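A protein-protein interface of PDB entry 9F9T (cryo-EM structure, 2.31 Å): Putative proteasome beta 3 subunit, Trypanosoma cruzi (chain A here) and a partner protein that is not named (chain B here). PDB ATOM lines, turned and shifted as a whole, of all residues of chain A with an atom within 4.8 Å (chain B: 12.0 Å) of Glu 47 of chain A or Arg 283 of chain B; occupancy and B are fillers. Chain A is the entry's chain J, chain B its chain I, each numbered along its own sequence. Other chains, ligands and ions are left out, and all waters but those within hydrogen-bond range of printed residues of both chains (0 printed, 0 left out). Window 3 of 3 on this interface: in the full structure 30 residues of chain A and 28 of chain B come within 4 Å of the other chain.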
ATOM      1  N   VAL A  44      25.542 -32.310  22.547  1.00  0.00           N
ATOM      2  CA  VAL A  44      24.945 -31.690  23.701  1.00  0.00           C
ATOM      3  C   VAL A  44      23.406 -31.851  23.675  1.00  0.00           C
ATOM      4  O   VAL A  44      22.694 -31.251  22.889  1.00  0.00           O
ATOM      5  CB  VAL A  44      25.376 -30.223  23.723  1.00  0.00           C
ATOM      6  CG1 VAL A  44      24.530 -29.380  24.659  1.00  0.00           C
ATOM      7  CG2 VAL A  44      26.841 -30.101  24.138  1.00  0.00           C
ATOM      8  N   ASN A  46      21.136 -31.163  26.504  1.00  0.00           N
ATOM      9  CA  ASN A  46      20.620 -29.951  27.110  1.00  0.00           C
ATOM     10  C   ASN A  46      21.695 -29.347  28.022  1.00  0.00           C
ATOM     11  O   ASN A  46      22.870 -29.648  27.943  1.00  0.00           O
ATOM     12  CB  ASN A  46      19.297 -30.223  27.798  1.00  0.00           C
ATOM     13  CG  ASN A  46      19.353 -31.271  28.894  1.00  0.00           C
ATOM     14  OD1 ASN A  46      20.306 -31.324  29.668  1.00  0.00           O
ATOM     15  ND2 ASN A  46      18.341 -32.124  28.964  1.00  0.00           N
ATOM     16  N   GLU A  47      21.344 -28.445  28.901  1.00  0.00           N
ATOM     17  CA  GLU A  47      22.371 -27.707  29.611  1.00  0.00           C
ATOM     18  C   GLU A  47      23.177 -28.606  30.529  1.00  0.00           C
ATOM     19  O   GLU A  47      24.296 -28.250  30.879  1.00  0.00           O
ATOM     20  CB  GLU A  47      21.695 -26.598  30.425  1.00  0.00           C
ATOM     21  CG  GLU A  47      21.323 -25.367  29.584  1.00  0.00           C
ATOM     22  CD  GLU A  47      20.905 -24.159  30.423  1.00  0.00           C
ATOM     23  OE1 GLU A  47      20.593 -24.356  31.624  1.00  0.00           O
ATOM     24  OE2 GLU A  47      20.937 -23.011  29.899  1.00  0.00           O
ATOM     25  N   SER A  48      22.586 -29.753  30.878  1.00  0.00           N
ATOM     26  CA  SER A  48      23.048 -30.658  31.925  1.00  0.00           C
ATOM     27  C   SER A  48      23.631 -31.944  31.365  1.00  0.00           C
ATOM     28  O   SER A  48      24.246 -32.650  32.154  1.00  0.00           O
ATOM     29  CB  SER A  48      21.897 -31.061  32.882  1.00  0.00           C
ATOM     30  OG  SER A  48      21.530 -30.000  33.764  1.00  0.00           O
ATOM     31  N   ILE A  49      23.308 -32.325  30.115  1.00  0.00           N
ATOM     32  CA  ILE A  49      23.672 -33.662  29.656  1.00  0.00           C
ATOM     33  C   ILE A  49      24.555 -33.606  28.407  1.00  0.00           C
ATOM     34  O   ILE A  49      24.188 -32.934  27.435  1.00  0.00           O
ATOM     35  CB  ILE A  49      22.422 -34.518  29.386  1.00  0.00           C
ATOM     36  CG1 ILE A  49      21.573 -34.804  30.618  1.00  0.00           C
ATOM     37  CG2 ILE A  49      22.879 -35.831  28.775  1.00  0.00           C
ATOM     38  CD1 ILE A  49      20.190 -35.334  30.258  1.00  0.00           C
ATOM     39  N   VAL A 190      31.660 -29.033  32.390  1.00  0.00           N
ATOM     40  CA  VAL A 190      30.312 -28.642  32.766  1.00  0.00           C
ATOM     41  C   VAL A 190      30.293 -28.538  34.282  1.00  0.00           C
ATOM     42  O   VAL A 190      30.870 -29.375  34.981  1.00  0.00           O
ATOM     43  CB  VAL A 190      29.212 -29.590  32.201  1.00  0.00           C
ATOM     44  CG1 VAL A 190      27.784 -29.259  32.617  1.00  0.00           C
ATOM     45  CG2 VAL A 190      29.264 -29.693  30.694  1.00  0.00           C
ATOM     46  N   ASP A 193      26.739 -24.049  36.636  1.00  0.00           N
ATOM     47  CA  ASP A 193      26.671 -22.649  36.240  1.00  0.00           C
ATOM     48  C   ASP A 193      27.201 -22.408  34.831  1.00  0.00           C
ATOM     49  O   ASP A 193      26.744 -21.452  34.207  1.00  0.00           O
ATOM     50  CB  ASP A 193      27.436 -21.753  37.227  1.00  0.00           C
ATOM     51  CG  ASP A 193      26.772 -21.636  38.599  1.00  0.00           C
ATOM     52  OD1 ASP A 193      25.742 -22.317  38.826  1.00  0.00           O
ATOM     53  OD2 ASP A 193      27.273 -20.851  39.445  1.00  0.00           O
ATOM     54  N   LYS A 194      28.224 -23.150  34.354  1.00  0.00           N
ATOM     55  CA  LYS A 194      28.719 -22.876  33.009  1.00  0.00           C
ATOM     56  C   LYS A 194      29.178 -24.126  32.272  1.00  0.00           C
ATOM     57  O   LYS A 194      29.329 -25.178  32.863  1.00  0.00           O
ATOM     58  CB  LYS A 194      29.719 -21.721  33.003  1.00  0.00           C
ATOM     59  CG  LYS A 194      31.123 -21.964  33.515  1.00  0.00           C
ATOM     60  CD  LYS A 194      32.013 -20.767  33.173  1.00  0.00           C
ATOM     61  CE  LYS A 194      33.037 -20.433  34.245  1.00  0.00           C
ATOM     62  NZ  LYS A 194      34.423 -20.802  33.866  1.00  0.00           N
ATOM     63  N   MET A 195      29.291 -23.994  30.952  1.00  0.00           N
ATOM     64  CA  MET A 195      29.733 -25.038  30.030  1.00  0.00           C
ATOM     65  C   MET A 195      30.796 -24.456  29.119  1.00  0.00           C
ATOM     66  O   MET A 195      30.538 -23.573  28.307  1.00  0.00           O
ATOM     67  CB  MET A 195      28.590 -25.595  29.164  1.00  0.00           C
ATOM     68  CG  MET A 195      29.060 -26.117  27.806  1.00  0.00           C
ATOM     69  SD  MET A 195      28.191 -27.577  27.142  1.00  0.00           S
ATOM     70  CE  MET A 195      26.525 -27.272  27.759  1.00  0.00           C
ATOM     71  N   ARG B 279      41.885 -23.358  21.278  1.00  0.00           N
ATOM     72  CA  ARG B 279      40.644 -22.605  21.164  1.00  0.00           C
ATOM     73  C   ARG B 279      39.685 -22.943  22.300  1.00  0.00           C
ATOM     74  O   ARG B 279      39.576 -24.084  22.720  1.00  0.00           O
ATOM     75  CB  ARG B 279      39.997 -22.869  19.807  1.00  0.00           C
ATOM     76  CG  ARG B 279      40.325 -21.834  18.739  1.00  0.00           C
ATOM     77  CD  ARG B 279      39.710 -22.182  17.385  1.00  0.00           C
ATOM     78  NE  ARG B 279      38.290 -21.830  17.308  1.00  0.00           N
ATOM     79  CZ  ARG B 279      37.421 -22.334  16.429  1.00  0.00           C
ATOM     80  NH1 ARG B 279      36.214 -21.806  16.315  1.00  0.00           N
ATOM     81  NH2 ARG B 279      37.773 -23.338  15.638  1.00  0.00           N
ATOM     82  N   GLU B 280      38.941 -21.929  22.747  1.00  0.00           N
ATOM     83  CA  GLU B 280      38.093 -22.028  23.928  1.00  0.00           C
ATOM     84  C   GLU B 280      36.775 -21.325  23.628  1.00  0.00           C
ATOM     85  O   GLU B 280      36.780 -20.278  22.995  1.00  0.00           O
ATOM     86  CB  GLU B 280      38.829 -21.408  25.126  1.00  0.00           C
ATOM     87  CG  GLU B 280      38.054 -21.442  26.443  1.00  0.00           C
ATOM     88  CD  GLU B 280      38.864 -21.216  27.726  1.00  0.00           C
ATOM     89  OE1 GLU B 280      39.905 -21.905  27.930  1.00  0.00           O
ATOM     90  OE2 GLU B 280      38.436 -20.376  28.553  1.00  0.00           O
ATOM     91  N   GLU B 281      35.662 -21.877  24.099  1.00  0.00           N
ATOM     92  CA  GLU B 281      34.416 -21.128  24.158  1.00  0.00           C
ATOM     93  C   GLU B 281      33.736 -21.347  25.505  1.00  0.00           C
ATOM     94  O   GLU B 281      33.905 -22.392  26.116  1.00  0.00           O
ATOM     95  CB  GLU B 281      33.498 -21.510  22.995  1.00  0.00           C
ATOM     96  CG  GLU B 281      34.006 -21.030  21.632  1.00  0.00           C
ATOM     97  CD  GLU B 281      33.204 -21.478  20.411  1.00  0.00           C
ATOM     98  OE1 GLU B 281      32.241 -22.280  20.575  1.00  0.00           O
ATOM     99  OE2 GLU B 281      33.545 -21.024  19.284  1.00  0.00           O
ATOM    100  N   ILE B 282      32.932 -20.366  25.934  1.00  0.00           N
ATOM    101  CA  ILE B 282      32.241 -20.389  27.222  1.00  0.00           C
ATOM    102  C   ILE B 282      30.757 -20.145  26.999  1.00  0.00           C
ATOM    103  O   ILE B 282      30.350 -19.614  25.970  1.00  0.00           O
ATOM    104  CB  ILE B 282      32.856 -19.369  28.201  1.00  0.00           C
ATOM    105  CG1 ILE B 282      34.383 -19.528  28.278  1.00  0.00           C
ATOM    106  CG2 ILE B 282      32.189 -19.488  29.561  1.00  0.00           C
ATOM    107  CD1 ILE B 282      35.067 -18.722  29.367  1.00  0.00           C
ATOM    108  N   ARG B 283      29.947 -20.636  27.932  1.00  0.00           N
ATOM    109  CA  ARG B 283      28.499 -20.588  27.818  1.00  0.00           C
ATOM    110  C   ARG B 283      27.968 -20.525  29.247  1.00  0.00           C
ATOM    111  O   ARG B 283      28.220 -21.446  30.019  1.00  0.00           O
ATOM    112  CB  ARG B 283      28.005 -21.809  27.018  1.00  0.00           C
ATOM    113  CG  ARG B 283      26.843 -21.553  26.058  1.00  0.00           C
ATOM    114  CD  ARG B 283      26.243 -22.808  25.411  1.00  0.00           C
ATOM    115  NE  ARG B 283      24.986 -23.309  25.995  1.00  0.00           N
ATOM    116  CZ  ARG B 283      24.379 -24.461  25.662  1.00  0.00           C
ATOM    117  NH1 ARG B 283      23.247 -24.814  26.251  1.00  0.00           N
ATOM    118  NH2 ARG B 283      24.904 -25.275  24.757  1.00  0.00           N
ATOM    119  N   ARG B 284      27.275 -19.431  29.600  1.00  0.00           N
ATOM    120  CA  ARG B 284      26.708 -19.241  30.934  1.00  0.00           C
ATOM    121  C   ARG B 284      25.342 -19.929  31.050  1.00  0.00           C
ATOM    122  O   ARG B 284      24.471 -19.741  30.192  1.00  0.00           O
ATOM    123  CB  ARG B 284      26.548 -17.747  31.238  1.00  0.00           C
ATOM    124  CG  ARG B 284      27.859 -16.979  31.304  1.00  0.00           C
ATOM    125  CD  ARG B 284      28.607 -17.200  32.605  1.00  0.00           C
ATOM    126  NE  ARG B 284      30.006 -16.816  32.486  1.00  0.00           N
ATOM    127  CZ  ARG B 284      30.920 -17.011  33.434  1.00  0.00           C
ATOM    128  NH1 ARG B 284      30.554 -17.432  34.634  1.00  0.00           N
ATOM    129  NH2 ARG B 284      32.198 -16.773  33.182  1.00  0.00           N
ATOM    130  N   LEU B 285      25.164 -20.713  32.132  1.00  0.00           N
ATOM    131  CA  LEU B 285      23.936 -21.468  32.362  1.00  0.00           C
ATOM    132  C   LEU B 285      23.115 -20.839  33.507  1.00  0.00           C
ATOM    133  O   LEU B 285      23.123 -19.593  33.644  1.00  0.00           O
ATOM    134  CB  LEU B 285      24.269 -22.940  32.676  1.00  0.00           C
ATOM    135  CG  LEU B 285      25.189 -23.698  31.706  1.00  0.00           C
ATOM    136  CD1 LEU B 285      24.980 -25.205  31.813  1.00  0.00           C
ATOM    137  CD2 LEU B 285      25.017 -23.266  30.258  1.00  0.00           C
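The backbone carbonyl oxygen (O) of Arg 283 of chain B sits at hydrogen-bond distance from the backbone NH (N) of Met 195 of chain A, 2.9 Å away. N of Leu 285 of chain B sits at hydrogen-bond distance from O of Asp 193 of chain A, at 2.7 Å.
Arg 283 of chain B touches Glu 47 of chain A. Leu 285 of chain B touches Glu 47 of chain A (CD1 to O, 3.3 Å). Arg 284 of chain B touches Asp 193 of chain A. CG2 of Ile 282 of chain B touches CD of Lys 194 of chain A, at 3.8 Å. CB of Lys 194 of chain A touches O of Arg 283 of chain B (3.4 Å). CE of Lys 194 of chain A touches NH2 of Arg 284 of chain B, 3.9 Å away. CG of Leu 285 of chain B touches CA of Lys 194 of chain A (3.9 Å). Ile 282 of chain B touches Met 195 of chain A (C to O, 3.7 Å).
No residue of chain B comes within 4 Å of Val 44 of chain A. No residue of chain B comes within 4 Å of Asn 46 of chain A. No residue of chain B comes within 4 Å of Ser 48 of chain A. No residue of chain B comes within 4 Å of Ile 49 of chain A. No residue of chain B comes within 4 Å of Val 190 of chain A. Of the printed residues of chain B, Asp 193 of chain A touches Arg 284 (3.8 Å) and Leu 285 (2.7 Å). Of chain B, only Ile 282, Arg 283, Arg 284 and Leu 285 come within 4 Å of Lys 194 of chain A. Met 195 of chain A touches two residues of chain B. Arg 279 of chain B touches none of the printed residues of chain A. Glu 280 of chain B touches none of the printed residues of chain A. Printed residues of chain A within 4 Å of Ile 282 of chain B: Lys 194 (3.8 Å) and Met 195 (3.7 Å). Arg 283 of chain B touches just these residues of chain A: Glu 47 (3.9 Å), Lys 194 (3.4 Å) and Met 195 (2.9 Å). Of the printed residues of chain A, Arg 284 of chain B touches Asp 193 (3.8 Å) and Lys 194 (3.9 Å). Of the printed residues of chain A, Leu 285 of chain B touches Glu 47, Asp 193 and Lys 194. The nearest residue of chain B that does not touch Glu 47 of chain A is Arg 284 of chain B (4.8 Å). The nearest residue of chain A that does not touch Arg 283 of chain B is Val 44 of chain A (4.1 Å). The nearest printed residue of chain B that does not touch Asp 193 of chain A is Arg 283 of chain B (4.4 Å).
Of the 9 printed residues of chain A, 4 touch a printed residue of chain B. Printed residues of chain A that touch a printed residue of chain B: Glu 47, Asp 193, Lys 194 and Met 195. Hydrophobic or aromatic side chains of chain B that line the printed part of chain A: Ile 282 and Leu 285.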
